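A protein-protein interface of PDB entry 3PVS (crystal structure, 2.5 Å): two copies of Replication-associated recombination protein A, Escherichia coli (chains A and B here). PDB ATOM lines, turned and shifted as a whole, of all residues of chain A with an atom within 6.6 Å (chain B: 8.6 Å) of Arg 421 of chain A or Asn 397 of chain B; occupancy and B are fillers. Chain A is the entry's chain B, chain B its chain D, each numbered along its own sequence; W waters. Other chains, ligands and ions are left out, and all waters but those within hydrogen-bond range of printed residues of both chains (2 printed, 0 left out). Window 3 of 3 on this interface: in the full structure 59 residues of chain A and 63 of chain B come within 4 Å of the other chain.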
ATOM      1  N   ASN A 305     -12.659  -0.644  16.541  1.00  0.00           N
ATOM      2  CA  ASN A 305     -13.762  -1.117  17.359  1.00  0.00           C
ATOM      3  C   ASN A 305     -14.911  -1.764  16.598  1.00  0.00           C
ATOM      4  O   ASN A 305     -15.936  -2.070  17.196  1.00  0.00           O
ATOM      5  CB  ASN A 305     -14.222  -0.031  18.327  1.00  0.00           C
ATOM      6  CG  ASN A 305     -13.141   0.352  19.320  1.00  0.00           C
ATOM      7  OD1 ASN A 305     -12.262  -0.450  19.642  1.00  0.00           O
ATOM      8  ND2 ASN A 305     -13.180   1.585  19.797  1.00  0.00           N
ATOM      9  N   ALA A 306     -14.736  -1.993  15.293  1.00  0.00           N
ATOM     10  CA  ALA A 306     -15.510  -3.035  14.592  1.00  0.00           C
ATOM     11  C   ALA A 306     -15.221  -4.392  15.225  1.00  0.00           C
ATOM     12  O   ALA A 306     -16.101  -5.277  15.218  1.00  0.00           O
ATOM     13  CB  ALA A 306     -15.170  -3.082  13.140  1.00  0.00           C
ATOM     14  N   ASP A 307     -14.004  -4.552  15.786  1.00  0.00           N
ATOM     15  CA  ASP A 307     -13.668  -5.733  16.609  1.00  0.00           C
ATOM     16  C   ASP A 307     -12.490  -5.522  17.574  1.00  0.00           C
ATOM     17  O   ASP A 307     -11.358  -5.803  17.252  1.00  0.00           O
ATOM     18  CB  ASP A 307     -13.480  -6.974  15.720  1.00  0.00           C
ATOM     19  CG  ASP A 307     -12.902  -8.145  16.453  1.00  0.00           C
ATOM     20  OD1 ASP A 307     -13.188  -8.369  17.664  1.00  0.00           O
ATOM     21  OD2 ASP A 307     -12.134  -8.843  15.787  1.00  0.00           O
ATOM     22  N   PRO A 344     -13.802  -7.712  10.424  1.00  0.00           N
ATOM     23  CA  PRO A 344     -14.512  -6.569   9.896  1.00  0.00           C
ATOM     24  C   PRO A 344     -13.626  -5.323  10.011  1.00  0.00           C
ATOM     25  O   PRO A 344     -12.866  -5.175  10.992  1.00  0.00           O
ATOM     26  CB  PRO A 344     -15.755  -6.461  10.789  1.00  0.00           C
ATOM     27  CG  PRO A 344     -15.384  -7.161  12.056  1.00  0.00           C
ATOM     28  CD  PRO A 344     -14.453  -8.251  11.640  1.00  0.00           C
ATOM     29  N   LYS A 345     -13.735  -4.446   9.011  1.00  0.00           N
ATOM     30  CA  LYS A 345     -12.778  -3.411   8.794  1.00  0.00           C
ATOM     31  C   LYS A 345     -13.373  -2.086   9.168  1.00  0.00           C
ATOM     32  O   LYS A 345     -14.527  -1.812   8.844  1.00  0.00           O
ATOM     33  CB  LYS A 345     -12.342  -3.413   7.318  1.00  0.00           C
ATOM     34  CG  LYS A 345     -11.490  -4.639   6.908  1.00  0.00           C
ATOM     35  CD  LYS A 345     -10.344  -4.957   7.934  1.00  0.00           C
ATOM     36  CE  LYS A 345      -9.450  -6.147   7.519  1.00  0.00           C
ATOM     37  NZ  LYS A 345     -10.258  -7.399   7.262  1.00  0.00           N
ATOM     38  N   SER A 346     -12.595  -1.263   9.874  1.00  0.00           N
ATOM     39  CA  SER A 346     -13.044   0.083  10.205  1.00  0.00           C
ATOM     40  C   SER A 346     -11.848   0.919  10.550  1.00  0.00           C
ATOM     41  O   SER A 346     -11.126   0.574  11.464  1.00  0.00           O
ATOM     42  CB  SER A 346     -13.979   0.094  11.422  1.00  0.00           C
ATOM     43  OG  SER A 346     -14.073   1.425  11.948  1.00  0.00           O
ATOM     44  N   ASN A 347     -11.664   2.021   9.838  1.00  0.00           N
ATOM     45  CA  ASN A 347     -10.636   2.976  10.173  1.00  0.00           C
ATOM     46  C   ASN A 347     -11.205   4.161  10.966  1.00  0.00           C
ATOM     47  O   ASN A 347     -10.579   5.244  10.988  1.00  0.00           O
ATOM     48  CB  ASN A 347      -9.928   3.465   8.920  1.00  0.00           C
ATOM     49  CG  ASN A 347     -10.797   4.435   8.073  1.00  0.00           C
ATOM     50  OD1 ASN A 347     -10.258   5.231   7.317  1.00  0.00           O
ATOM     51  ND2 ASN A 347     -12.126   4.329   8.172  1.00  0.00           N
ATOM     52  N   PRO A 418     -18.772   5.863  13.643  1.00  0.00           N
ATOM     53  CA  PRO A 418     -18.629   4.388  13.553  1.00  0.00           C
ATOM     54  C   PRO A 418     -19.165   3.824  12.225  1.00  0.00           C
ATOM     55  O   PRO A 418     -20.127   4.398  11.640  1.00  0.00           O
ATOM     56  CB  PRO A 418     -19.434   3.871  14.751  1.00  0.00           C
ATOM     57  CG  PRO A 418     -20.224   5.028  15.245  1.00  0.00           C
ATOM     58  CD  PRO A 418     -19.550   6.291  14.813  1.00  0.00           C
ATOM     59  N   THR A 419     -18.545   2.763  11.714  1.00  0.00           N
ATOM     60  CA  THR A 419     -19.008   2.215  10.455  1.00  0.00           C
ATOM     61  C   THR A 419     -20.195   1.348  10.823  1.00  0.00           C
ATOM     62  O   THR A 419     -20.562   1.316  11.993  1.00  0.00           O
ATOM     63  CB  THR A 419     -17.967   1.309   9.834  1.00  0.00           C
ATOM     64  OG1 THR A 419     -17.926   0.093  10.591  1.00  0.00           O
ATOM     65  CG2 THR A 419     -16.619   1.984   9.772  1.00  0.00           C
ATOM     66  N   ASN A 420     -20.762   0.595   9.887  1.00  0.00           N
ATOM     67  CA  ASN A 420     -21.803  -0.384  10.268  1.00  0.00           C
ATOM     68  C   ASN A 420     -21.305  -1.852  10.276  1.00  0.00           C
ATOM     69  O   ASN A 420     -22.105  -2.796  10.260  1.00  0.00           O
ATOM     70  CB  ASN A 420     -23.079  -0.212   9.405  1.00  0.00           C
ATOM     71  CG  ASN A 420     -22.887  -0.706   7.957  1.00  0.00           C
ATOM     72  OD1 ASN A 420     -21.787  -1.072   7.554  1.00  0.00           O
ATOM     73  ND2 ASN A 420     -23.966  -0.744   7.192  1.00  0.00           N
ATOM     74  N   ARG A 421     -19.984  -2.042  10.290  1.00  0.00           N
ATOM     75  CA  ARG A 421     -19.413  -3.391  10.287  1.00  0.00           C
ATOM     76  C   ARG A 421     -19.021  -3.875  11.678  1.00  0.00           C
ATOM     77  O   ARG A 421     -18.650  -3.077  12.531  1.00  0.00           O
ATOM     78  CB  ARG A 421     -18.193  -3.409   9.411  1.00  0.00           C
ATOM     79  CG  ARG A 421     -18.442  -3.167   7.943  1.00  0.00           C
ATOM     80  CD  ARG A 421     -17.229  -2.420   7.293  1.00  0.00           C
ATOM     81  NE  ARG A 421     -17.775  -1.383   6.431  1.00  0.00           N
ATOM     82  CZ  ARG A 421     -17.307  -0.155   6.229  1.00  0.00           C
ATOM     83  NH1 ARG A 421     -16.224   0.301   6.821  1.00  0.00           N
ATOM     84  NH2 ARG A 421     -17.971   0.635   5.395  1.00  0.00           N
ATOM     85  N   GLY A 422     -19.078  -5.192  11.897  1.00  0.00           N
ATOM     86  CA  GLY A 422     -18.742  -5.795  13.178  1.00  0.00           C
ATOM     87  C   GLY A 422     -19.470  -5.165  14.357  1.00  0.00           C
ATOM     88  O   GLY A 422     -20.679  -4.937  14.334  1.00  0.00           O
ATOM     89  N   LEU A 423     -18.728  -4.844  15.401  1.00  0.00           N
ATOM     90  CA  LEU A 423     -19.346  -4.323  16.615  1.00  0.00           C
ATOM     91  C   LEU A 423     -19.883  -2.887  16.480  1.00  0.00           C
ATOM     92  O   LEU A 423     -20.706  -2.449  17.293  1.00  0.00           O
ATOM     93  CB  LEU A 423     -18.313  -4.351  17.734  1.00  0.00           C
ATOM     94  CG  LEU A 423     -18.846  -4.855  19.046  1.00  0.00           C
ATOM     95  CD1 LEU A 423     -18.957  -6.441  18.944  1.00  0.00           C
ATOM     96  CD2 LEU A 423     -17.854  -4.371  20.092  1.00  0.00           C
ATOM     97  N   GLU A 424     -19.393  -2.155  15.481  1.00  0.00           N
ATOM     98  CA  GLU A 424     -19.739  -0.755  15.330  1.00  0.00           C
ATOM     99  C   GLU A 424     -21.185  -0.506  14.846  1.00  0.00           C
ATOM    100  O   GLU A 424     -21.635   0.629  14.822  1.00  0.00           O
ATOM    101  CB  GLU A 424     -18.710  -0.008  14.455  1.00  0.00           C
ATOM    102  CG  GLU A 424     -17.396   0.367  15.153  1.00  0.00           C
ATOM    103  CD  GLU A 424     -16.455   1.186  14.259  1.00  0.00           C
ATOM    104  OE1 GLU A 424     -15.656   1.989  14.765  1.00  0.00           O
ATOM    105  OE2 GLU A 424     -16.506   1.065  13.029  1.00  0.00           O
ATOM    106  N   GLY A 425     -21.907  -1.558  14.463  1.00  0.00           N
ATOM    107  CA  GLY A 425     -23.322  -1.407  14.121  1.00  0.00           C
ATOM    108  C   GLY A 425     -24.075  -1.032  15.396  1.00  0.00           C
ATOM    109  O   GLY A 425     -24.742   0.011  15.470  1.00  0.00           O
ATOM    110  N   ALA B 392      -8.913   0.445   0.639  1.00  0.00           N
ATOM    111  CA  ALA B 392     -10.108  -0.356   0.802  1.00  0.00           C
ATOM    112  C   ALA B 392     -11.235   0.346   1.587  1.00  0.00           C
ATOM    113  O   ALA B 392     -12.415   0.120   1.317  1.00  0.00           O
ATOM    114  CB  ALA B 392      -9.721  -1.710   1.422  1.00  0.00           C
ATOM    115  N   HIS B 393     -10.855   1.197   2.552  1.00  0.00           N
ATOM    116  CA  HIS B 393     -11.805   1.901   3.420  1.00  0.00           C
ATOM    117  C   HIS B 393     -12.699   2.853   2.650  1.00  0.00           C
ATOM    118  O   HIS B 393     -13.850   2.992   3.000  1.00  0.00           O
ATOM    119  CB  HIS B 393     -11.094   2.660   4.537  1.00  0.00           C
ATOM    120  CG  HIS B 393     -10.390   1.772   5.515  1.00  0.00           C
ATOM    121  ND1 HIS B 393     -11.072   0.950   6.392  1.00  0.00           N
ATOM    122  CD2 HIS B 393      -9.065   1.553   5.735  1.00  0.00           C
ATOM    123  CE1 HIS B 393     -10.197   0.263   7.104  1.00  0.00           C
ATOM    124  NE2 HIS B 393      -8.976   0.598   6.717  1.00  0.00           N
ATOM    125  N   ASP B 394     -12.182   3.487   1.602  1.00  0.00           N
ATOM    126  CA  ASP B 394     -12.964   4.416   0.751  1.00  0.00           C
ATOM    127  C   ASP B 394     -13.906   3.746  -0.290  1.00  0.00           C
ATOM    128  O   ASP B 394     -14.520   4.440  -1.093  1.00  0.00           O
ATOM    129  CB  ASP B 394     -12.022   5.398   0.022  1.00  0.00           C
ATOM    130  CG  ASP B 394     -11.312   6.325   0.978  1.00  0.00           C
ATOM    131  OD1 ASP B 394     -11.802   6.485   2.094  1.00  0.00           O
ATOM    132  OD2 ASP B 394     -10.268   6.902   0.647  1.00  0.00           O
ATOM    133  N   GLU B 395     -14.008   2.421  -0.288  1.00  0.00           N
ATOM    134  CA  GLU B 395     -14.857   1.725  -1.227  1.00  0.00           C
ATOM    135  C   GLU B 395     -16.026   1.096  -0.523  1.00  0.00           C
ATOM    136  O   GLU B 395     -16.064   1.059   0.714  1.00  0.00           O
ATOM    137  CB  GLU B 395     -14.062   0.668  -1.957  1.00  0.00           C
ATOM    138  CG  GLU B 395     -13.035   1.338  -2.850  1.00  0.00           C
ATOM    139  CD  GLU B 395     -12.590   0.495  -4.048  1.00  0.00           C
ATOM    140  OE1 GLU B 395     -13.355  -0.389  -4.508  1.00  0.00           O
ATOM    141  OE2 GLU B 395     -11.477   0.754  -4.529  1.00  0.00           O
ATOM    142  N   ALA B 396     -16.982   0.597  -1.293  1.00  0.00           N
ATOM    143  CA  ALA B 396     -18.194   0.030  -0.701  1.00  0.00           C
ATOM    144  C   ALA B 396     -17.809  -1.099   0.260  1.00  0.00           C
ATOM    145  O   ALA B 396     -17.002  -1.955  -0.082  1.00  0.00           O
ATOM    146  CB  ALA B 396     -19.172  -0.484  -1.806  1.00  0.00           C
ATOM    147  N   ASN B 397     -18.371  -1.081   1.463  1.00  0.00           N
ATOM    148  CA  ASN B 397     -18.188  -2.176   2.410  1.00  0.00           C
ATOM    149  C   ASN B 397     -16.752  -2.296   2.909  1.00  0.00           C
ATOM    150  O   ASN B 397     -16.427  -3.251   3.605  1.00  0.00           O
ATOM    151  CB  ASN B 397     -18.646  -3.495   1.798  1.00  0.00           C
ATOM    152  CG  ASN B 397     -20.142  -3.522   1.555  1.00  0.00           C
ATOM    153  OD1 ASN B 397     -20.931  -2.997   2.368  1.00  0.00           O
ATOM    154  ND2 ASN B 397     -20.554  -4.117   0.431  1.00  0.00           N
ATOM    155  N   ALA B 398     -15.905  -1.313   2.569  1.00  0.00           N
ATOM    156  CA  ALA B 398     -14.494  -1.328   2.933  1.00  0.00           C
ATOM    157  C   ALA B 398     -13.807  -2.561   2.319  1.00  0.00           C
ATOM    158  O   ALA B 398     -12.860  -3.134   2.875  1.00  0.00           O
ATOM    159  CB  ALA B 398     -14.312  -1.262   4.448  1.00  0.00           C
ATOM    160  N   TYR B 399     -14.325  -2.960   1.161  1.00  0.00           N
ATOM    161  CA  TYR B 399     -13.716  -4.016   0.380  1.00  0.00           C
ATOM    162  C   TYR B 399     -13.416  -3.546  -1.022  1.00  0.00           C
ATOM    163  O   TYR B 399     -14.249  -2.935  -1.651  1.00  0.00           O
ATOM    164  CB  TYR B 399     -14.640  -5.189   0.336  1.00  0.00           C
ATOM    165  CG  TYR B 399     -14.021  -6.435  -0.185  1.00  0.00           C
ATOM    166  CD1 TYR B 399     -14.503  -7.010  -1.356  1.00  0.00           C
ATOM    167  CD2 TYR B 399     -12.983  -7.089   0.510  1.00  0.00           C
ATOM    168  CE1 TYR B 399     -13.969  -8.181  -1.838  1.00  0.00           C
ATOM    169  CE2 TYR B 399     -12.454  -8.271   0.025  1.00  0.00           C
ATOM    170  CZ  TYR B 399     -12.961  -8.805  -1.160  1.00  0.00           C
ATOM    171  OH  TYR B 399     -12.491  -9.994  -1.680  1.00  0.00           O
ATOM    172  N   ALA B 400     -12.211  -3.797  -1.511  1.00  0.00           N
ATOM    173  CA  ALA B 400     -11.837  -3.290  -2.828  1.00  0.00           C
ATOM    174  C   ALA B 400     -12.147  -4.395  -3.833  1.00  0.00           C
ATOM    175  O   ALA B 400     -11.242  -5.072  -4.322  1.00  0.00           O
ATOM    176  CB  ALA B 400     -10.384  -2.936  -2.854  1.00  0.00           C
ATOM    177  N   ALA B 401     -13.445  -4.565  -4.109  1.00  0.00           N
ATOM    178  CA  ALA B 401     -13.935  -5.684  -4.902  1.00  0.00           C
ATOM    179  C   ALA B 401     -13.177  -5.752  -6.207  1.00  0.00           C
ATOM    180  O   ALA B 401     -12.975  -4.717  -6.884  1.00  0.00           O
ATOM    181  CB  ALA B 401     -15.438  -5.598  -5.132  1.00  0.00           C
ATOM    182  N   LYS B 430     -18.346 -15.299   5.198  1.00  0.00           N
ATOM    183  CA  LYS B 430     -17.825 -13.989   4.840  1.00  0.00           C
ATOM    184  C   LYS B 430     -16.937 -14.090   3.613  1.00  0.00           C
ATOM    185  O   LYS B 430     -17.052 -13.260   2.739  1.00  0.00           O
ATOM    186  CB  LYS B 430     -17.075 -13.319   5.998  1.00  0.00           C
ATOM    187  CG  LYS B 430     -16.911 -11.815   5.847  1.00  0.00           C
ATOM    188  CD  LYS B 430     -15.655 -11.305   6.480  1.00  0.00           C
ATOM    189  CE  LYS B 430     -15.785  -9.843   6.960  1.00  0.00           C
ATOM    190  NZ  LYS B 430     -14.522  -9.022   6.739  1.00  0.00           N
ATOM    191  N   TRP B 433     -19.007 -14.666   0.422  1.00  0.00           N
ATOM    192  CA  TRP B 433     -19.588 -13.400   0.043  1.00  0.00           C
ATOM    193  C   TRP B 433     -18.566 -12.385  -0.532  1.00  0.00           C
ATOM    194  O   TRP B 433     -18.853 -11.667  -1.493  1.00  0.00           O
ATOM    195  CB  TRP B 433     -20.320 -12.828   1.241  1.00  0.00           C
ATOM    196  CG  TRP B 433     -21.115 -11.609   0.928  1.00  0.00           C
ATOM    197  CD1 TRP B 433     -22.324 -11.560   0.310  1.00  0.00           C
ATOM    198  CD2 TRP B 433     -20.755 -10.249   1.220  1.00  0.00           C
ATOM    199  NE1 TRP B 433     -22.752 -10.251   0.200  1.00  0.00           N
ATOM    200  CE2 TRP B 433     -21.807  -9.428   0.753  1.00  0.00           C
ATOM    201  CE3 TRP B 433     -19.647  -9.645   1.835  1.00  0.00           C
ATOM    202  CZ2 TRP B 433     -21.786  -8.027   0.881  1.00  0.00           C
ATOM    203  CZ3 TRP B 433     -19.627  -8.245   1.969  1.00  0.00           C
ATOM    204  CH2 TRP B 433     -20.683  -7.456   1.485  1.00  0.00           C
ATOM    205  N   LEU B 434     -17.373 -12.312   0.040  1.00  0.00           N
ATOM    206  CA  LEU B 434     -16.322 -11.483  -0.568  1.00  0.00           C
ATOM    207  C   LEU B 434     -15.977 -11.947  -1.991  1.00  0.00           C
ATOM    208  O   LEU B 434     -15.861 -11.134  -2.907  1.00  0.00           O
ATOM    209  CB  LEU B 434     -15.054 -11.425   0.310  1.00  0.00           C
ATOM    210  CG  LEU B 434     -15.241 -10.861   1.723  1.00  0.00           C
ATOM    211  CD1 LEU B 434     -14.031 -11.082   2.538  1.00  0.00           C
ATOM    212  CD2 LEU B 434     -15.538  -9.415   1.675  1.00  0.00           C
ATOM    213  N   GLN B 437     -18.477 -10.627  -4.446  1.00  0.00           N
ATOM    214  CA  GLN B 437     -18.184  -9.215  -4.711  1.00  0.00           C
ATOM    215  C   GLN B 437     -17.048  -9.076  -5.731  1.00  0.00           C
ATOM    216  O   GLN B 437     -17.063  -8.153  -6.524  1.00  0.00           O
ATOM    217  CB  GLN B 437     -17.785  -8.438  -3.439  1.00  0.00           C
ATOM    218  CG  GLN B 437     -18.793  -8.372  -2.324  1.00  0.00           C
ATOM    219  CD  GLN B 437     -20.178  -8.054  -2.811  1.00  0.00           C
ATOM    220  OE1 GLN B 437     -21.049  -8.942  -2.846  1.00  0.00           O
ATOM    221  NE2 GLN B 437     -20.403  -6.802  -3.222  1.00  0.00           N
HETATM  222  O   HOH W   1     -17.145   2.706   2.994  1.00  0.00           O
HETATM  223  O   HOH W   2     -13.576   1.565   7.419  1.00  0.00           O
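Water W2 lies within hydrogen-bond range of a ring nitrogen (ND1) of His 393 of chain B (2.8 Å), the guanidinium group of Arg 421 of chain A (3.0 Å) and the backbone NH of Asn 347 of chain A (3.1 Å).
Water W1 lies within hydrogen-bond range of the backbone carbonyl oxygen of Glu 395 of chain B (3.0 Å), the guanidinium group of Arg 421 of chain A (3.3 Å) and the backbone carbonyl oxygen of His 393 of chain B (3.3 Å).
The backbone carbonyl oxygen (O) of Lys 345 of chain A lies close to the guanidinium group (NH1) of Arg 421 of chain A, 3.4 Å away.
OG1 of Thr 419 of chain A sits at hydrogen-bond distance from N of Arg 421 of chain A, at 3.0 Å.
OG of Ser 346 of chain A lies within hydrogen-bond range of OE2 of Glu 424 of chain A (2.7 Å).
No position is printed for both chains.
Of the 5 pairs that touch across the chains among the printed residues, none has its exchanged pair printed and touching as well.
Among the printed residues, pairs that only touch across the chains: Pro 344 of chain A with Lys 430 of chain B (3.98 Å), Ser 346 of chain A with His 393 of chain B (3.9 Å), Asn 347 of chain A with His 393 of chain B (3.6 Å), Arg 421 of chain A with Asn 397 of chain B (3.6 Å) and Arg 421 of chain A with Ala 398 of chain B (3.4 Å).
Of the 15 printed residues of chain A, 4 touch a printed residue of chain B.
Along chain B the printed residues that touch a printed residue of chain A span positions 393 to 430.
Among the printed residues, no Asp or Glu carboxylate lies within 4 Å of a Lys or Arg side-chain nitrogen of the other chain.
Of the printed residues of chain B, Pro 344 of chain A touches Lys 430 (3.98 Å).
Lys 345 of chain A touches none of the printed residues of chain B.
Of the printed residues of chain B, Ser 346 of chain A touches His 393 (3.9 Å).
Of chain B, only Asn 397 and Ala 398 come within 4 Å of Arg 421 of chain A.
No residue of chain B comes within 4 Å of Gly 422 of chain A.
Of the printed residues of chain A, His 393 of chain B touches Ser 346 and Asn 347.
Asn 397 of chain B touches just one residue of chain A: Arg 421.
Of the printed residues of chain A, Ala 398 of chain B touches Arg 421.
Ala 400 of chain B touches none of the printed residues of chain A.
The nearest residue of chain B that does not touch Arg 421 of chain A is Glu 395 of chain B (5.1 Å).
The nearest residue of chain A that does not touch Asn 397 of chain B is Lys 345 of chain A (5.5 Å).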
